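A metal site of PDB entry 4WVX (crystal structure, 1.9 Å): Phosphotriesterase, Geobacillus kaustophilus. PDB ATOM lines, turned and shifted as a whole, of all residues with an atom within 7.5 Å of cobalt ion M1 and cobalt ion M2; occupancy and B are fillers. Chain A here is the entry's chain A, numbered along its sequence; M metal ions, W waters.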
ATOM      1  N   HIS A  23      11.746  20.052  -5.863  1.00  0.00           N
ATOM      2  CA  HIS A  23      13.218  20.089  -5.750  1.00  0.00           C
ATOM      3  C   HIS A  23      13.898  19.782  -7.063  1.00  0.00           C
ATOM      4  O   HIS A  23      14.144  18.613  -7.376  1.00  0.00           O
ATOM      5  CB  HIS A  23      13.667  19.085  -4.699  1.00  0.00           C
ATOM      6  CG  HIS A  23      15.080  19.268  -4.230  1.00  0.00           C
ATOM      7  ND1 HIS A  23      15.391  19.329  -2.891  1.00  0.00           N
ATOM      8  CD2 HIS A  23      16.250  19.374  -4.889  1.00  0.00           C
ATOM      9  CE1 HIS A  23      16.684  19.465  -2.741  1.00  0.00           C
ATOM     10  NE2 HIS A  23      17.243  19.491  -3.943  1.00  0.00           N
ATOM     11  N   GLU A  24      14.220  20.831  -7.820  1.00  0.00           N
ATOM     12  CA  GLU A  24      14.998  20.677  -9.052  1.00  0.00           C
ATOM     13  C   GLU A  24      15.958  21.836  -9.194  1.00  0.00           C
ATOM     14  O   GLU A  24      15.679  22.932  -8.727  1.00  0.00           O
ATOM     15  CB  GLU A  24      14.099  20.665 -10.286  1.00  0.00           C
ATOM     16  CG  GLU A  24      12.887  19.736 -10.233  1.00  0.00           C
ATOM     17  CD  GLU A  24      13.234  18.268 -10.406  1.00  0.00           C
ATOM     18  OE1 GLU A  24      14.325  17.934 -10.919  1.00  0.00           O
ATOM     19  OE2 GLU A  24      12.389  17.444 -10.000  1.00  0.00           O
ATOM     20  N   HIS A  25      17.089  21.605  -9.856  1.00  0.00           N
ATOM     21  CA  HIS A  25      18.046  22.679 -10.158  1.00  0.00           C
ATOM     22  C   HIS A  25      18.150  23.024 -11.623  1.00  0.00           C
ATOM     23  O   HIS A  25      18.451  22.165 -12.458  1.00  0.00           O
ATOM     24  CB  HIS A  25      19.454  22.345  -9.684  1.00  0.00           C
ATOM     25  CG  HIS A  25      19.490  21.952  -8.257  1.00  0.00           C
ATOM     26  ND1 HIS A  25      19.581  22.867  -7.232  1.00  0.00           N
ATOM     27  CD2 HIS A  25      19.390  20.741  -7.671  1.00  0.00           C
ATOM     28  CE1 HIS A  25      19.559  22.235  -6.076  1.00  0.00           C
ATOM     29  NE2 HIS A  25      19.430  20.940  -6.317  1.00  0.00           N
ATOM     30  N   PHE A  28      23.615  24.286 -11.222  1.00  0.00           N
ATOM     31  CA  PHE A  28      24.270  23.866 -10.000  1.00  0.00           C
ATOM     32  C   PHE A  28      25.753  23.709 -10.242  1.00  0.00           C
ATOM     33  O   PHE A  28      26.146  23.193 -11.295  1.00  0.00           O
ATOM     34  CB  PHE A  28      23.671  22.539  -9.506  1.00  0.00           C
ATOM     35  CG  PHE A  28      24.197  22.109  -8.164  1.00  0.00           C
ATOM     36  CD1 PHE A  28      25.356  21.364  -8.078  1.00  0.00           C
ATOM     37  CD2 PHE A  28      23.540  22.459  -6.997  1.00  0.00           C
ATOM     38  CE1 PHE A  28      25.864  20.985  -6.858  1.00  0.00           C
ATOM     39  CE2 PHE A  28      24.044  22.079  -5.764  1.00  0.00           C
ATOM     40  CZ  PHE A  28      25.212  21.337  -5.704  1.00  0.00           C
ATOM     41  N   ASP A  68      13.461  25.596  -6.750  1.00  0.00           N
ATOM     42  CA  ASP A  68      14.857  25.421  -7.086  1.00  0.00           C
ATOM     43  C   ASP A  68      15.653  25.892  -5.842  1.00  0.00           C
ATOM     44  O   ASP A  68      15.853  27.008  -5.587  1.00  0.00           O
ATOM     45  CB  ASP A  68      15.231  26.143  -8.371  1.00  0.00           C
ATOM     46  CG  ASP A  68      16.739  26.075  -8.694  1.00  0.00           C
ATOM     47  OD1 ASP A  68      17.553  25.972  -7.767  1.00  0.00           O
ATOM     48  OD2 ASP A  68      17.065  26.128  -9.854  1.00  0.00           O
ATOM     49  N   PRO A  69      16.102  24.909  -5.098  1.00  0.00           N
ATOM     50  CA  PRO A  69      16.717  25.161  -3.812  1.00  0.00           C
ATOM     51  C   PRO A  69      18.262  25.171  -3.940  1.00  0.00           C
ATOM     52  O   PRO A  69      18.906  24.701  -3.073  1.00  0.00           O
ATOM     53  CB  PRO A  69      16.208  24.009  -2.967  1.00  0.00           C
ATOM     54  CG  PRO A  69      16.140  22.883  -3.892  1.00  0.00           C
ATOM     55  CD  PRO A  69      15.836  23.487  -5.265  1.00  0.00           C
ATOM     56  N   THR A  70      18.798  25.640  -5.051  1.00  0.00           N
ATOM     57  CA  THR A  70      20.243  25.719  -5.229  1.00  0.00           C
ATOM     58  C   THR A  70      20.845  26.577  -4.104  1.00  0.00           C
ATOM     59  O   THR A  70      20.451  27.729  -3.936  1.00  0.00           O
ATOM     60  CB  THR A  70      20.610  26.332  -6.589  1.00  0.00           C
ATOM     61  OG1 THR A  70      20.049  25.527  -7.634  1.00  0.00           O
ATOM     62  CG2 THR A  70      22.096  26.343  -6.768  1.00  0.00           C
ATOM     63  N   PRO A  71      21.781  26.005  -3.325  1.00  0.00           N
ATOM     64  CA  PRO A  71      22.408  26.791  -2.244  1.00  0.00           C
ATOM     65  C   PRO A  71      23.212  27.991  -2.715  1.00  0.00           C
ATOM     66  O   PRO A  71      23.744  27.997  -3.830  1.00  0.00           O
ATOM     67  CB  PRO A  71      23.352  25.796  -1.589  1.00  0.00           C
ATOM     68  CG  PRO A  71      22.750  24.457  -1.874  1.00  0.00           C
ATOM     69  CD  PRO A  71      22.208  24.596  -3.275  1.00  0.00           C
ATOM     70  N   TYR A  99      25.074  25.068   1.610  1.00  0.00           N
ATOM     71  CA  TYR A  99      25.054  23.618   1.528  1.00  0.00           C
ATOM     72  C   TYR A  99      25.709  22.971   2.757  1.00  0.00           C
ATOM     73  O   TYR A  99      26.185  23.670   3.655  1.00  0.00           O
ATOM     74  CB  TYR A  99      25.794  23.209   0.278  1.00  0.00           C
ATOM     75  CG  TYR A  99      25.383  21.927  -0.364  1.00  0.00           C
ATOM     76  CD1 TYR A  99      24.066  21.433  -0.355  1.00  0.00           C
ATOM     77  CD2 TYR A  99      26.346  21.213  -1.030  1.00  0.00           C
ATOM     78  CE1 TYR A  99      23.769  20.233  -1.016  1.00  0.00           C
ATOM     79  CE2 TYR A  99      26.071  20.048  -1.679  1.00  0.00           C
ATOM     80  CZ  TYR A  99      24.804  19.550  -1.676  1.00  0.00           C
ATOM     81  OH  TYR A  99      24.657  18.345  -2.344  1.00  0.00           O
ATOM     82  N   TYR A 100      25.703  21.636   2.827  1.00  0.00           N
ATOM     83  CA  TYR A 100      26.302  20.949   3.972  1.00  0.00           C
ATOM     84  C   TYR A 100      27.826  21.061   3.915  1.00  0.00           C
ATOM     85  O   TYR A 100      28.427  21.352   2.877  1.00  0.00           O
ATOM     86  CB  TYR A 100      25.811  19.490   4.106  1.00  0.00           C
ATOM     87  CG  TYR A 100      26.397  18.503   3.141  1.00  0.00           C
ATOM     88  CD1 TYR A 100      25.988  18.454   1.821  1.00  0.00           C
ATOM     89  CD2 TYR A 100      27.342  17.562   3.575  1.00  0.00           C
ATOM     90  CE1 TYR A 100      26.539  17.527   0.956  1.00  0.00           C
ATOM     91  CE2 TYR A 100      27.894  16.640   2.718  1.00  0.00           C
ATOM     92  CZ  TYR A 100      27.477  16.619   1.406  1.00  0.00           C
ATOM     93  OH  TYR A 100      28.015  15.697   0.552  1.00  0.00           O
ATOM     94  N   KCX A 145      16.934  27.001   2.489  1.00  0.00           N
ATOM     95  CA  KCX A 145      17.546  25.675   2.275  1.00  0.00           C
ATOM     96  CB  KCX A 145      18.257  25.697   0.924  1.00  0.00           C
ATOM     97  CG  KCX A 145      19.124  24.472   0.683  1.00  0.00           C
ATOM     98  CD  KCX A 145      18.271  23.234   0.515  1.00  0.00           C
ATOM     99  CE  KCX A 145      19.090  22.025   0.130  1.00  0.00           C
ATOM    100  NZ  KCX A 145      19.386  22.059  -1.284  1.00  0.00           N
ATOM    101  C   KCX A 145      18.530  25.362   3.362  1.00  0.00           C
ATOM    102  O   KCX A 145      19.416  26.166   3.655  1.00  0.00           O
ATOM    103  CX  KCX A 145      19.734  20.954  -1.931  1.00  0.00           C
ATOM    104  OQ1 KCX A 145      19.851  19.871  -1.384  1.00  0.00           O
ATOM    105  OQ2 KCX A 145      19.978  21.033  -3.224  1.00  0.00           O
ATOM    106  N   LEU A 146      18.394  24.190   3.953  1.00  0.00           N
ATOM    107  CA  LEU A 146      19.286  23.692   4.988  1.00  0.00           C
ATOM    108  C   LEU A 146      19.855  22.374   4.541  1.00  0.00           C
ATOM    109  O   LEU A 146      19.223  21.647   3.765  1.00  0.00           O
ATOM    110  CB  LEU A 146      18.514  23.485   6.306  1.00  0.00           C
ATOM    111  CG  LEU A 146      18.022  24.722   7.036  1.00  0.00           C
ATOM    112  CD1 LEU A 146      17.278  24.311   8.320  1.00  0.00           C
ATOM    113  CD2 LEU A 146      19.179  25.671   7.320  1.00  0.00           C
ATOM    114  N   ALA A 147      21.025  22.044   5.059  1.00  0.00           N
ATOM    115  CA  ALA A 147      21.646  20.791   4.682  1.00  0.00           C
ATOM    116  C   ALA A 147      22.512  20.233   5.792  1.00  0.00           C
ATOM    117  O   ALA A 147      23.211  20.978   6.465  1.00  0.00           O
ATOM    118  CB  ALA A 147      22.460  21.016   3.441  1.00  0.00           C
ATOM    119  N   THR A 177      15.081  20.873   3.229  1.00  0.00           N
ATOM    120  CA  THR A 177      16.387  20.338   3.639  1.00  0.00           C
ATOM    121  C   THR A 177      16.960  19.311   2.665  1.00  0.00           C
ATOM    122  O   THR A 177      16.252  18.719   1.831  1.00  0.00           O
ATOM    123  CB  THR A 177      16.397  19.685   5.037  1.00  0.00           C
ATOM    124  OG1 THR A 177      15.883  18.342   4.964  1.00  0.00           O
ATOM    125  CG2 THR A 177      15.623  20.507   6.069  1.00  0.00           C
ATOM    126  N   HIS A 178      18.272  19.124   2.818  1.00  0.00           N
ATOM    127  CA  HIS A 178      19.068  18.070   2.238  1.00  0.00           C
ATOM    128  C   HIS A 178      19.473  17.170   3.397  1.00  0.00           C
ATOM    129  O   HIS A 178      19.980  17.657   4.405  1.00  0.00           O
ATOM    130  CB  HIS A 178      20.296  18.717   1.588  1.00  0.00           C
ATOM    131  CG  HIS A 178      21.433  17.797   1.301  1.00  0.00           C
ATOM    132  ND1 HIS A 178      21.821  17.498   0.013  1.00  0.00           N
ATOM    133  CD2 HIS A 178      22.327  17.179   2.113  1.00  0.00           C
ATOM    134  CE1 HIS A 178      22.871  16.702   0.040  1.00  0.00           C
ATOM    135  NE2 HIS A 178      23.198  16.492   1.303  1.00  0.00           N
ATOM    136  N   THR A 179      19.158  15.880   3.286  1.00  0.00           N
ATOM    137  CA  THR A 179      19.810  14.858   4.106  1.00  0.00           C
ATOM    138  C   THR A 179      20.838  14.115   3.271  1.00  0.00           C
ATOM    139  O   THR A 179      20.633  13.867   2.064  1.00  0.00           O
ATOM    140  CB  THR A 179      18.812  13.850   4.679  1.00  0.00           C
ATOM    141  OG1 THR A 179      18.113  13.185   3.630  1.00  0.00           O
ATOM    142  CG2 THR A 179      17.843  14.565   5.593  1.00  0.00           C
ATOM    143  N   GLN A 180      21.951  13.750   3.901  1.00  0.00           N
ATOM    144  CA  GLN A 180      23.048  13.102   3.198  1.00  0.00           C
ATOM    145  C   GLN A 180      22.993  11.578   3.412  1.00  0.00           C
ATOM    146  O   GLN A 180      23.003  11.088   4.549  1.00  0.00           O
ATOM    147  CB  GLN A 180      24.391  13.665   3.674  1.00  0.00           C
ATOM    148  CG  GLN A 180      25.628  13.195   2.927  1.00  0.00           C
ATOM    149  CD  GLN A 180      25.695  13.539   1.455  1.00  0.00           C
ATOM    150  OE1 GLN A 180      25.027  14.451   0.950  1.00  0.00           O
ATOM    151  NE2 GLN A 180      26.558  12.812   0.752  1.00  0.00           N
ATOM    152  N   GLY A 205      14.291  16.669   3.122  1.00  0.00           N
ATOM    153  CA  GLY A 205      14.613  16.222   1.780  1.00  0.00           C
ATOM    154  C   GLY A 205      15.468  14.975   1.706  1.00  0.00           C
ATOM    155  O   GLY A 205      16.094  14.558   2.685  1.00  0.00           O
ATOM    156  N   HIS A 206      15.524  14.436   0.493  1.00  0.00           N
ATOM    157  CA  HIS A 206      16.282  13.240   0.134  1.00  0.00           C
ATOM    158  C   HIS A 206      15.973  12.059   1.002  1.00  0.00           C
ATOM    159  O   HIS A 206      16.844  11.229   1.264  1.00  0.00           O
ATOM    160  CB  HIS A 206      17.802  13.500   0.106  1.00  0.00           C
ATOM    161  CG  HIS A 206      18.191  14.705  -0.671  1.00  0.00           C
ATOM    162  ND1 HIS A 206      17.452  15.172  -1.745  1.00  0.00           N
ATOM    163  CD2 HIS A 206      19.240  15.570  -0.533  1.00  0.00           C
ATOM    164  CE1 HIS A 206      18.028  16.255  -2.242  1.00  0.00           C
ATOM    165  NE2 HIS A 206      19.128  16.497  -1.539  1.00  0.00           N
ATOM    166  N   ASP A 229      12.839  12.881  -3.489  1.00  0.00           N
ATOM    167  CA  ASP A 229      13.129  13.962  -4.412  1.00  0.00           C
ATOM    168  C   ASP A 229      14.346  13.695  -5.289  1.00  0.00           C
ATOM    169  O   ASP A 229      14.816  14.602  -5.948  1.00  0.00           O
ATOM    170  CB  ASP A 229      13.266  15.279  -3.646  1.00  0.00           C
ATOM    171  CG  ASP A 229      14.289  15.221  -2.541  1.00  0.00           C
ATOM    172  OD1 ASP A 229      15.156  14.328  -2.605  1.00  0.00           O
ATOM    173  OD2 ASP A 229      14.242  16.060  -1.626  1.00  0.00           O
ATOM    174  N   ARG A 230      14.821  12.446  -5.318  1.00  0.00           N
ATOM    175  CA  ARG A 230      15.936  12.075  -6.188  1.00  0.00           C
ATOM    176  C   ARG A 230      15.646  10.921  -7.158  1.00  0.00           C
ATOM    177  O   ARG A 230      16.546  10.153  -7.514  1.00  0.00           O
ATOM    178  CB  ARG A 230      17.151  11.741  -5.346  1.00  0.00           C
ATOM    179  CG  ARG A 230      17.751  12.967  -4.711  1.00  0.00           C
ATOM    180  CD  ARG A 230      18.957  12.630  -3.842  1.00  0.00           C
ATOM    181  NE  ARG A 230      19.871  13.777  -3.805  1.00  0.00           N
ATOM    182  CZ  ARG A 230      21.008  13.841  -3.107  1.00  0.00           C
ATOM    183  NH1 ARG A 230      21.405  12.826  -2.347  1.00  0.00           N
ATOM    184  NH2 ARG A 230      21.750  14.960  -3.157  1.00  0.00           N
ATOM    185  N   HIS A 265      12.991  15.027  -8.657  1.00  0.00           N
ATOM    186  CA  HIS A 265      14.172  14.356  -9.181  1.00  0.00           C
ATOM    187  C   HIS A 265      15.522  14.933  -8.739  1.00  0.00           C
ATOM    188  O   HIS A 265      16.539  14.245  -8.901  1.00  0.00           O
ATOM    189  CB  HIS A 265      14.235  14.421 -10.720  1.00  0.00           C
ATOM    190  CG  HIS A 265      12.937  14.195 -11.439  1.00  0.00           C
ATOM    191  ND1 HIS A 265      12.049  15.215 -11.695  1.00  0.00           N
ATOM    192  CD2 HIS A 265      12.441  13.105 -12.053  1.00  0.00           C
ATOM    193  CE1 HIS A 265      11.028  14.750 -12.393  1.00  0.00           C
ATOM    194  NE2 HIS A 265      11.250  13.469 -12.635  1.00  0.00           N
ATOM    195  N   ASP A 266      15.575  16.183  -8.296  1.00  0.00           N
ATOM    196  CA  ASP A 266      16.851  16.822  -7.926  1.00  0.00           C
ATOM    197  C   ASP A 266      17.773  16.917  -9.164  1.00  0.00           C
ATOM    198  O   ASP A 266      18.987  16.766  -9.065  1.00  0.00           O
ATOM    199  CB  ASP A 266      17.509  16.047  -6.762  1.00  0.00           C
ATOM    200  CG  ASP A 266      18.620  16.827  -6.030  1.00  0.00           C
ATOM    201  OD1 ASP A 266      18.691  18.049  -6.171  1.00  0.00           O
ATOM    202  OD2 ASP A 266      19.400  16.195  -5.297  1.00  0.00           O
ATOM    203  N   THR A 267      17.181  17.184 -10.328  1.00  0.00           N
ATOM    204  CA  THR A 267      17.960  17.335 -11.543  1.00  0.00           C
ATOM    205  C   THR A 267      18.937  18.495 -11.429  1.00  0.00           C
ATOM    206  O   THR A 267      18.712  19.471 -10.699  1.00  0.00           O
ATOM    207  CB  THR A 267      17.126  17.556 -12.820  1.00  0.00           C
ATOM    208  OG1 THR A 267      16.233  18.673 -12.675  1.00  0.00           O
ATOM    209  CG2 THR A 267      16.376  16.259 -13.191  1.00  0.00           C
ATOM    210  N   VAL A 268      20.032  18.331 -12.150  1.00  0.00           N
ATOM    211  CA  VAL A 268      20.883  19.444 -12.471  1.00  0.00           C
ATOM    212  C   VAL A 268      20.852  19.641 -13.970  1.00  0.00           C
ATOM    213  O   VAL A 268      21.501  18.898 -14.714  1.00  0.00           O
ATOM    214  CB  VAL A 268      22.308  19.209 -11.988  1.00  0.00           C
ATOM    215  CG1 VAL A 268      23.222  20.346 -12.427  1.00  0.00           C
ATOM    216  CG2 VAL A 268      22.307  19.096 -10.477  1.00  0.00           C
HETATM  217 CO    CO M   1      19.336  19.549  -4.685  1.00  0.00          CO
HETATM  218 CO    CO M   2      20.685  18.039  -1.798  1.00  0.00          CO
HETATM  219  O   HOH W   1      20.385  18.084  -3.800  1.00  0.00           O
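Merely in contact with cobalt ion M2: Tyr 99 (3.9 Å) and Arg 230 (3.5 Å). Within 4 Å of cobalt ion M2: Tyr 99, KCX 145, His 178, His 206 and Arg 230. The nearest printed residue that does not touch cobalt ion M2 is Asp 266 (4.2 Å).
Cobalt ion M1 is bound by water W1. Cobalt ion M1 is bound by NE2 of His 25 (2.1 Å). OQ2 of KCX 145 is bound to cobalt ion M1 (2.2 Å). Cobalt ion M1 is bound by the side-chain carboxylate (OD1) of Asp 266. Cobalt ion M1 is bound by a ring nitrogen (NE2) of His 23, 2.2 Å away.
Of the 25 residues printed, 4 come within 4 Å of cobalt ion M1. The nearest printed residue that does not touch cobalt ion M1 is His 206 (4.3 Å).
Water W1 lies within hydrogen-bond range of the side-chain carboxylate (OD2) of Asp 266 (2.6 Å) and the guanidinium group (NH2) of Arg 230 (3.5 Å).
Water W1 binds cobalt ion M2 (2.0 Å). OQ1 of KCX 145 binds cobalt ion M2, at 2.1 Å. ND1 of His 178 is bound to cobalt ion M2. Cobalt ion M2 is bound by a ring nitrogen (NE2) of His 206, at 2.2 Å. Cobalt ion M2 has four donor atoms within binding distance.
NZ of KCX 145 is in hydrogen-bond range of the backbone carbonyl oxygen (O) of Pro 69 (3.2 Å). The backbone NH of His 25 sits at hydrogen-bond distance from the backbone carbonyl oxygen of Thr 267 (2.8 Å). ND1 of His 25 is in hydrogen-bond range of OG1 of Thr 70 (2.7 Å). A ring nitrogen (NE2) of His 178 lies within hydrogen-bond range of the side-chain amide oxygen of Gln 180 (2.8 Å). ND1 of His 206 sits close to NE of Arg 230, 3.5 Å away. OD1 of Asp 229 is in hydrogen-bond range of ND1 of His 206 (2.6 Å). The side-chain carboxylate (OD2) of Asp 266 is in salt-bridge range of the guanidinium group (NE) of Arg 230, at 2.9 Å. N of Asp 266 lies within hydrogen-bond range of OE1 of Glu 24 (3.4 Å).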
